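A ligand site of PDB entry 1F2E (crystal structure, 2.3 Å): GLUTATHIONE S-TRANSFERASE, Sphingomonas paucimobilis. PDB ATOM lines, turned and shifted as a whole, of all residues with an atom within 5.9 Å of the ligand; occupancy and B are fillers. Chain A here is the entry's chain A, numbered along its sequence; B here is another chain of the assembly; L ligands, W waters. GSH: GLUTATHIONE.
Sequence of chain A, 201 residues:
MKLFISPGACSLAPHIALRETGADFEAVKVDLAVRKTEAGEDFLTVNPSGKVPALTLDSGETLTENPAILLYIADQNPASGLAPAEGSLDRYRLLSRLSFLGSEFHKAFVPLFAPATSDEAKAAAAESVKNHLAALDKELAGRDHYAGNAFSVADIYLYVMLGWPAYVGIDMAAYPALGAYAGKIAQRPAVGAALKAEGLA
Water W5 lies within hydrogen-bond range of the side-chain hydroxyl of Ser 99 of chain B, an oxygen (O11) of the ligand, the side-chain carboxylate of Glu 65 and the side-chain hydroxyl of Ser 103 of chain B.
Water W1 lies within hydrogen-bond range of O of Gly 102, N1 of the ligand and ND1 of His 106.
Water W3 lies within hydrogen-bond range of the guanidinium group (NE) of Arg 35, the backbone carbonyl oxygen (O) of Gly 50 and an oxygen (O32) of the ligand.
Water W6 lies within hydrogen-bond range of the backbone carbonyl oxygen of Pro 53, the backbone NH of Glu 65 and an oxygen (O12) of the ligand.
Water W2 lies within hydrogen-bond range of the side-chain hydroxyl (OH) of Tyr 157 (2.4 Å), a ring nitrogen (ND1) of His 106 (2.6 Å), the side-chain amide nitrogen (ND2) of Asn 66 (3.1 Å) and an oxygen (O11) of the ligand (3.1 Å).
Water W4 lies within hydrogen-bond range of OE1 of Glu 65 (2.7 Å) and OE1 of Glu 104 of chain B (3.0 Å).
The side-chain hydroxyl (OG) of Ser 103 of chain B sits at hydrogen-bond distance from a nitrogen (N1) of the ligand, 3.0 Å away.
A nitrogen (N2) of the ligand is in hydrogen-bond range of the backbone carbonyl oxygen (O) of Val 52 (2.8 Å).
OE1 of Glu 104 of chain B is in salt-bridge range of N1 of the ligand, at 2.8 Å.
The backbone NH of Val 52 sits at hydrogen-bond distance from an oxygen (O2) of the ligand (2.9 Å).
N of Cys 10 sits close to SG2 of the ligand (3.2 Å).
N of Asn 66 is in hydrogen-bond range of O12 of the ligand, 3.1 Å away.
The side-chain sulfur (SG) of Cys 10 is covalently linked to a sulfur (SG2) of the ligand, at 2.1 Å.
OE2 of Glu 65 is in salt-bridge range of N1 of the ligand (3.0 Å).
CB of Ala 9 touches SG2 of the ligand (3.99 Å).
CD1 of Leu 32 touches O2 of the ligand, at 3.8 Å.
Lys 51 touches the ligand (CA to O2, 3.3 Å).
Pro 53 touches the ligand.
CD of Pro 67 touches O11 of the ligand, at 3.8 Å.
His 106 touches the ligand (CE1 to OE1, 3.6 Å).
Tyr 157 touches the ligand.
Hydrophobic or aromatic side chains that line the ligand: Ala 9, Leu 32, Val 52, Pro 53, Pro 67 and His 106.
Of the 23 residues printed, 13 come within 4 Å of the ligand.
OE2 of Glu 104 of chain B lies within salt-bridge range of NZ of Lys 51 (3.6 Å).
ND2 of Asn 66 sits at hydrogen-bond distance from O of Cys 10 (3.4 Å).
The backbone carbonyl oxygen (O) of Leu 32 lies close to the guanidinium group (NE) of Arg 35, at 3.4 Å.
NZ of Lys 107 lies within salt-bridge range of OE2 of Glu 104 of chain B, at 3.0 Å.
OG of Ser 103 of chain B sits at hydrogen-bond distance from OE2 of Glu 65 (3.4 Å).
The side-chain hydroxyl (OG) of Ser 103 of chain B is in hydrogen-bond range of the backbone carbonyl oxygen (O) of Ser 99 of chain B (2.7 Å).
OE2 of Glu 65 lies within hydrogen-bond range of OG of Ser 99 of chain B, at 3.2 Å.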
ATOM      1  N   ALA A   9       1.295 -11.084 -15.890  1.00  0.00           N
ATOM      2  CA  ALA A   9       2.389 -10.146 -16.157  1.00  0.00           C
ATOM      3  C   ALA A   9       2.955  -9.560 -14.866  1.00  0.00           C
ATOM      4  O   ALA A   9       2.518  -9.890 -13.761  1.00  0.00           O
ATOM      5  CB  ALA A   9       1.899  -9.036 -17.085  1.00  0.00           C
ATOM      6  N   CYS A  10       3.939  -8.670 -15.020  1.00  0.00           N
ATOM      7  CA  CYS A  10       4.580  -8.019 -13.876  1.00  0.00           C
ATOM      8  C   CYS A  10       3.545  -7.256 -13.025  1.00  0.00           C
ATOM      9  O   CYS A  10       3.792  -6.945 -11.859  1.00  0.00           O
ATOM     10  CB  CYS A  10       5.648  -7.037 -14.381  1.00  0.00           C
ATOM     11  SG  CYS A  10       5.012  -5.972 -15.690  1.00  0.00           S
ATOM     12  N   SER A  11       2.388  -6.962 -13.608  1.00  0.00           N
ATOM     13  CA  SER A  11       1.338  -6.257 -12.885  1.00  0.00           C
ATOM     14  C   SER A  11       0.678  -7.145 -11.816  1.00  0.00           C
ATOM     15  O   SER A  11      -0.150  -6.673 -11.044  1.00  0.00           O
ATOM     16  CB  SER A  11       0.276  -5.724 -13.851  1.00  0.00           C
ATOM     17  OG  SER A  11      -0.317  -6.781 -14.577  1.00  0.00           O
ATOM     18  N   LEU A  32      -3.229  -5.978 -24.031  1.00  0.00           N
ATOM     19  CA  LEU A  32      -1.997  -5.335 -24.468  1.00  0.00           C
ATOM     20  C   LEU A  32      -1.783  -5.409 -25.970  1.00  0.00           C
ATOM     21  O   LEU A  32      -1.098  -4.564 -26.550  1.00  0.00           O
ATOM     22  CB  LEU A  32      -0.801  -5.927 -23.725  1.00  0.00           C
ATOM     23  CG  LEU A  32      -0.799  -5.636 -22.224  1.00  0.00           C
ATOM     24  CD1 LEU A  32       0.405  -6.276 -21.552  1.00  0.00           C
ATOM     25  CD2 LEU A  32      -0.801  -4.128 -22.006  1.00  0.00           C
ATOM     26  N   ALA A  33      -2.374  -6.413 -26.608  1.00  0.00           N
ATOM     27  CA  ALA A  33      -2.234  -6.589 -28.047  1.00  0.00           C
ATOM     28  C   ALA A  33      -2.799  -5.392 -28.807  1.00  0.00           C
ATOM     29  O   ALA A  33      -2.286  -5.015 -29.851  1.00  0.00           O
ATOM     30  CB  ALA A  33      -2.908  -7.876 -28.496  1.00  0.00           C
ATOM     31  N   ARG A  35      -4.025  -2.461 -26.873  1.00  0.00           N
ATOM     32  CA  ARG A  35      -4.075  -1.352 -25.924  1.00  0.00           C
ATOM     33  C   ARG A  35      -5.490  -0.863 -25.605  1.00  0.00           C
ATOM     34  O   ARG A  35      -5.782   0.325 -25.692  1.00  0.00           O
ATOM     35  CB  ARG A  35      -3.255  -0.173 -26.439  1.00  0.00           C
ATOM     36  CG  ARG A  35      -1.755  -0.309 -26.243  1.00  0.00           C
ATOM     37  CD  ARG A  35      -1.171  -1.445 -27.053  1.00  0.00           C
ATOM     38  NE  ARG A  35       0.290  -1.482 -26.963  1.00  0.00           N
ATOM     39  CZ  ARG A  35       1.089  -0.520 -27.430  1.00  0.00           C
ATOM     40  NH1 ARG A  35       0.574   0.548 -28.032  1.00  0.00           N
ATOM     41  NH2 ARG A  35       2.400  -0.618 -27.284  1.00  0.00           N
ATOM     42  N   GLY A  50       1.787   2.517 -22.803  1.00  0.00           N
ATOM     43  CA  GLY A  50       1.002   1.327 -23.091  1.00  0.00           C
ATOM     44  C   GLY A  50       1.352   0.133 -22.224  1.00  0.00           C
ATOM     45  O   GLY A  50       0.970  -0.994 -22.532  1.00  0.00           O
ATOM     46  N   LYS A  51       2.060   0.375 -21.125  1.00  0.00           N
ATOM     47  CA  LYS A  51       2.465  -0.722 -20.250  1.00  0.00           C
ATOM     48  C   LYS A  51       1.713  -0.786 -18.925  1.00  0.00           C
ATOM     49  O   LYS A  51       1.280   0.231 -18.376  1.00  0.00           O
ATOM     50  CB  LYS A  51       3.971  -0.631 -19.953  1.00  0.00           C
ATOM     51  CG  LYS A  51       4.850  -0.617 -21.189  1.00  0.00           C
ATOM     52  CD  LYS A  51       6.324  -0.692 -20.808  1.00  0.00           C
ATOM     53  CE  LYS A  51       7.205  -0.731 -22.051  1.00  0.00           C
ATOM     54  NZ  LYS A  51       8.633  -0.916 -21.703  1.00  0.00           N
ATOM     55  N   VAL A  52       1.579  -2.011 -18.409  1.00  0.00           N
ATOM     56  CA  VAL A  52       0.961  -2.222 -17.111  1.00  0.00           C
ATOM     57  C   VAL A  52       2.167  -2.615 -16.260  1.00  0.00           C
ATOM     58  O   VAL A  52       3.192  -3.033 -16.778  1.00  0.00           O
ATOM     59  CB  VAL A  52      -0.056  -3.390 -17.133  1.00  0.00           C
ATOM     60  CG1 VAL A  52      -1.203  -3.064 -18.066  1.00  0.00           C
ATOM     61  CG2 VAL A  52       0.640  -4.703 -17.553  1.00  0.00           C
ATOM     62  N   PRO A  53       2.068  -2.456 -14.933  1.00  0.00           N
ATOM     63  CA  PRO A  53       0.906  -1.948 -14.213  1.00  0.00           C
ATOM     64  C   PRO A  53       0.817  -0.439 -14.257  1.00  0.00           C
ATOM     65  O   PRO A  53       1.772   0.253 -14.615  1.00  0.00           O
ATOM     66  CB  PRO A  53       1.154  -2.439 -12.793  1.00  0.00           C
ATOM     67  CG  PRO A  53       2.640  -2.298 -12.681  1.00  0.00           C
ATOM     68  CD  PRO A  53       3.115  -2.897 -14.001  1.00  0.00           C
ATOM     69  N   THR A  64       2.815   5.115 -12.407  1.00  0.00           N
ATOM     70  CA  THR A  64       3.418   4.013 -13.155  1.00  0.00           C
ATOM     71  C   THR A  64       4.727   3.595 -12.496  1.00  0.00           C
ATOM     72  O   THR A  64       5.273   4.319 -11.646  1.00  0.00           O
ATOM     73  CB  THR A  64       3.696   4.381 -14.625  1.00  0.00           C
ATOM     74  OG1 THR A  64       4.608   5.478 -14.687  1.00  0.00           O
ATOM     75  CG2 THR A  64       2.397   4.738 -15.352  1.00  0.00           C
ATOM     76  N   GLU A  65       5.226   2.425 -12.901  1.00  0.00           N
ATOM     77  CA  GLU A  65       6.474   1.840 -12.403  1.00  0.00           C
ATOM     78  C   GLU A  65       6.217   1.085 -11.092  1.00  0.00           C
ATOM     79  O   GLU A  65       5.861   1.674 -10.085  1.00  0.00           O
ATOM     80  CB  GLU A  65       7.534   2.930 -12.224  1.00  0.00           C
ATOM     81  CG  GLU A  65       7.907   3.645 -13.540  1.00  0.00           C
ATOM     82  CD  GLU A  65       8.667   2.751 -14.516  1.00  0.00           C
ATOM     83  OE1 GLU A  65       8.571   2.989 -15.734  1.00  0.00           O
ATOM     84  OE2 GLU A  65       9.383   1.818 -14.070  1.00  0.00           O
ATOM     85  N   ASN A  66       6.418  -0.236 -11.136  1.00  0.00           N
ATOM     86  CA  ASN A  66       6.187  -1.099  -9.993  1.00  0.00           C
ATOM     87  C   ASN A  66       6.737  -0.659  -8.634  1.00  0.00           C
ATOM     88  O   ASN A  66       6.030  -0.703  -7.640  1.00  0.00           O
ATOM     89  CB  ASN A  66       6.654  -2.525 -10.295  1.00  0.00           C
ATOM     90  CG  ASN A  66       5.530  -3.423 -10.777  1.00  0.00           C
ATOM     91  OD1 ASN A  66       4.439  -3.411 -10.206  1.00  0.00           O
ATOM     92  ND2 ASN A  66       5.770  -4.187 -11.839  1.00  0.00           N
ATOM     93  N   PRO A  67       8.012  -0.226  -8.584  1.00  0.00           N
ATOM     94  CA  PRO A  67       8.512   0.189  -7.272  1.00  0.00           C
ATOM     95  C   PRO A  67       7.662   1.288  -6.648  1.00  0.00           C
ATOM     96  O   PRO A  67       7.300   1.216  -5.467  1.00  0.00           O
ATOM     97  CB  PRO A  67       9.937   0.667  -7.583  1.00  0.00           C
ATOM     98  CG  PRO A  67      10.320  -0.179  -8.793  1.00  0.00           C
ATOM     99  CD  PRO A  67       9.059  -0.118  -9.623  1.00  0.00           C
ATOM    100  N   GLY A 102      13.381  -4.404 -10.383  1.00  0.00           N
ATOM    101  CA  GLY A 102      12.806  -3.778 -11.569  1.00  0.00           C
ATOM    102  C   GLY A 102      13.802  -3.460 -12.684  1.00  0.00           C
ATOM    103  O   GLY A 102      13.464  -3.615 -13.863  1.00  0.00           O
ATOM    104  N   HIS A 106      14.009  -8.156 -13.594  1.00  0.00           N
ATOM    105  CA  HIS A 106      12.881  -8.099 -14.521  1.00  0.00           C
ATOM    106  C   HIS A 106      13.360  -7.896 -15.953  1.00  0.00           C
ATOM    107  O   HIS A 106      12.870  -8.546 -16.883  1.00  0.00           O
ATOM    108  CB  HIS A 106      11.925  -6.972 -14.109  1.00  0.00           C
ATOM    109  CG  HIS A 106      10.690  -6.886 -14.937  1.00  0.00           C
ATOM    110  ND1 HIS A 106       9.645  -6.025 -14.626  1.00  0.00           N
ATOM    111  CD2 HIS A 106      10.321  -7.508 -16.088  1.00  0.00           C
ATOM    112  CE1 HIS A 106       8.702  -6.127 -15.544  1.00  0.00           C
ATOM    113  NE2 HIS A 106       9.087  -7.029 -16.438  1.00  0.00           N
ATOM    114  N   LYS A 107      14.329  -7.005 -16.122  1.00  0.00           N
ATOM    115  CA  LYS A 107      14.838  -6.707 -17.460  1.00  0.00           C
ATOM    116  C   LYS A 107      15.592  -7.850 -18.123  1.00  0.00           C
ATOM    117  O   LYS A 107      15.630  -7.932 -19.358  1.00  0.00           O
ATOM    118  CB  LYS A 107      15.700  -5.441 -17.419  1.00  0.00           C
ATOM    119  CG  LYS A 107      14.844  -4.199 -17.197  1.00  0.00           C
ATOM    120  CD  LYS A 107      13.715  -4.147 -18.228  1.00  0.00           C
ATOM    121  CE  LYS A 107      12.783  -2.956 -18.053  1.00  0.00           C
ATOM    122  NZ  LYS A 107      11.801  -2.852 -19.172  1.00  0.00           N
ATOM    123  N   TYR A 157       7.003  -8.771  -5.155  1.00  0.00           N
ATOM    124  CA  TYR A 157       7.615  -8.414  -6.426  1.00  0.00           C
ATOM    125  C   TYR A 157       8.533  -9.550  -6.909  1.00  0.00           C
ATOM    126  O   TYR A 157       8.446 -10.002  -8.071  1.00  0.00           O
ATOM    127  CB  TYR A 157       8.405  -7.110  -6.238  1.00  0.00           C
ATOM    128  CG  TYR A 157       8.771  -6.343  -7.496  1.00  0.00           C
ATOM    129  CD1 TYR A 157       8.130  -6.564  -8.710  1.00  0.00           C
ATOM    130  CD2 TYR A 157       9.756  -5.345  -7.435  1.00  0.00           C
ATOM    131  CE1 TYR A 157       8.452  -5.813  -9.843  1.00  0.00           C
ATOM    132  CE2 TYR A 157      10.088  -4.589  -8.551  1.00  0.00           C
ATOM    133  CZ  TYR A 157       9.440  -4.820  -9.746  1.00  0.00           C
ATOM    134  OH  TYR A 157       9.800  -4.069 -10.840  1.00  0.00           O
ATOM    135  N   TRP A 164       8.295 -16.933 -13.504  1.00  0.00           N
ATOM    136  CA  TRP A 164       8.586 -16.930 -14.944  1.00  0.00           C
ATOM    137  C   TRP A 164       9.602 -17.921 -15.506  1.00  0.00           C
ATOM    138  O   TRP A 164       9.390 -18.507 -16.565  1.00  0.00           O
ATOM    139  CB  TRP A 164       8.995 -15.531 -15.397  1.00  0.00           C
ATOM    140  CG  TRP A 164       8.001 -14.445 -15.093  1.00  0.00           C
ATOM    141  CD1 TRP A 164       6.643 -14.574 -15.018  1.00  0.00           C
ATOM    142  CD2 TRP A 164       8.288 -13.058 -14.902  1.00  0.00           C
ATOM    143  NE1 TRP A 164       6.058 -13.350 -14.787  1.00  0.00           N
ATOM    144  CE2 TRP A 164       7.054 -12.399 -14.716  1.00  0.00           C
ATOM    145  CE3 TRP A 164       9.467 -12.303 -14.869  1.00  0.00           C
ATOM    146  CZ2 TRP A 164       6.958 -11.013 -14.501  1.00  0.00           C
ATOM    147  CZ3 TRP A 164       9.389 -10.927 -14.649  1.00  0.00           C
ATOM    148  CH2 TRP A 164       8.126 -10.297 -14.473  1.00  0.00           C
ATOM    149  N   SER B  99      12.587   5.423 -11.129  1.00  0.00           N
ATOM    150  CA  SER B  99      12.421   4.030 -11.529  1.00  0.00           C
ATOM    151  C   SER B  99      12.349   3.875 -13.047  1.00  0.00           C
ATOM    152  O   SER B  99      12.848   2.898 -13.611  1.00  0.00           O
ATOM    153  CB  SER B  99      11.156   3.477 -10.877  1.00  0.00           C
ATOM    154  OG  SER B  99      10.911   2.157 -11.305  1.00  0.00           O
ATOM    155  N   PHE B 100      11.734   4.831 -13.723  1.00  0.00           N
ATOM    156  CA  PHE B 100      11.654   4.767 -15.173  1.00  0.00           C
ATOM    157  C   PHE B 100      13.049   4.933 -15.757  1.00  0.00           C
ATOM    158  O   PHE B 100      13.428   4.242 -16.718  1.00  0.00           O
ATOM    159  CB  PHE B 100      10.760   5.873 -15.719  1.00  0.00           C
ATOM    160  CG  PHE B 100      10.811   6.008 -17.222  1.00  0.00           C
ATOM    161  CD1 PHE B 100      10.062   5.160 -18.038  1.00  0.00           C
ATOM    162  CD2 PHE B 100      11.629   6.964 -17.830  1.00  0.00           C
ATOM    163  CE1 PHE B 100      10.129   5.273 -19.436  1.00  0.00           C
ATOM    164  CE2 PHE B 100      11.701   7.079 -19.220  1.00  0.00           C
ATOM    165  CZ  PHE B 100      10.947   6.224 -20.030  1.00  0.00           C
ATOM    166  N   SER B 103      15.184   1.681 -14.872  1.00  0.00           N
ATOM    167  CA  SER B 103      14.778   0.430 -15.496  1.00  0.00           C
ATOM    168  C   SER B 103      14.517   0.480 -16.988  1.00  0.00           C
ATOM    169  O   SER B 103      14.674  -0.524 -17.674  1.00  0.00           O
ATOM    170  CB  SER B 103      13.549  -0.131 -14.777  1.00  0.00           C
ATOM    171  OG  SER B 103      12.393   0.629 -15.074  1.00  0.00           O
ATOM    172  N   GLU B 104      14.145   1.645 -17.512  1.00  0.00           N
ATOM    173  CA  GLU B 104      13.868   1.764 -18.935  1.00  0.00           C
ATOM    174  C   GLU B 104      14.957   2.525 -19.700  1.00  0.00           C
ATOM    175  O   GLU B 104      15.614   1.962 -20.573  1.00  0.00           O
ATOM    176  CB  GLU B 104      12.522   2.461 -19.164  1.00  0.00           C
ATOM    177  CG  GLU B 104      11.346   1.789 -18.474  1.00  0.00           C
ATOM    178  CD  GLU B 104      11.058   0.391 -19.007  1.00  0.00           C
ATOM    179  OE1 GLU B 104      10.224  -0.319 -18.413  1.00  0.00           O
ATOM    180  OE2 GLU B 104      11.651   0.015 -20.037  1.00  0.00           O
HETATM  181  N1  GSH L   1       9.800  -0.691 -15.620  1.00  0.00           N
HETATM  182  CA1 GSH L   1       8.344  -0.872 -15.617  1.00  0.00           C
HETATM  183  C1  GSH L   1       7.788  -1.151 -14.188  1.00  0.00           C
HETATM  184  O11 GSH L   1       8.596  -1.210 -13.212  1.00  0.00           O
HETATM  185  O12 GSH L   1       6.527  -1.293 -14.067  1.00  0.00           O
HETATM  186  CB1 GSH L   1       8.078  -2.046 -16.593  1.00  0.00           C
HETATM  187  CG1 GSH L   1       6.622  -2.422 -16.931  1.00  0.00           C
HETATM  188  CD1 GSH L   1       6.554  -3.579 -17.929  1.00  0.00           C
HETATM  189  OE1 GSH L   1       7.583  -4.153 -18.315  1.00  0.00           O
HETATM  190  N2  GSH L   1       5.323  -3.909 -18.359  1.00  0.00           N
HETATM  191  CA2 GSH L   1       5.047  -4.980 -19.330  1.00  0.00           C
HETATM  192  C2  GSH L   1       4.096  -4.473 -20.385  1.00  0.00           C
HETATM  193  O2  GSH L   1       3.034  -3.922 -20.045  1.00  0.00           O
HETATM  194  CB2 GSH L   1       4.382  -6.197 -18.662  1.00  0.00           C
HETATM  195  SG2 GSH L   1       5.348  -7.059 -17.426  1.00  0.00           S
HETATM  196  N3  GSH L   1       4.459  -4.637 -21.655  1.00  0.00           N
HETATM  197  CA3 GSH L   1       3.618  -4.167 -22.759  1.00  0.00           C
HETATM  198  C3  GSH L   1       3.370  -5.245 -23.766  1.00  0.00           C
HETATM  199  O31 GSH L   1       3.725  -6.430 -23.477  1.00  0.00           O
HETATM  200  O32 GSH L   1       2.820  -4.905 -24.847  1.00  0.00           O
HETATM  201  O   HOH W   1      11.033  -3.071 -14.973  1.00  0.00           O
HETATM  202  O   HOH W   2       8.637  -4.322 -12.944  1.00  0.00           O
HETATM  203  O   HOH W   3       1.659  -2.281 -24.864  1.00  0.00           O
HETATM  204  O   HOH W   4       7.967   1.615 -17.946  1.00  0.00           O
HETATM  205  O   HOH W   5      10.919  -0.038 -12.443  1.00  0.00           O
HETATM  206  O   HOH W   6       4.468   0.574 -14.822  1.00  0.00           O
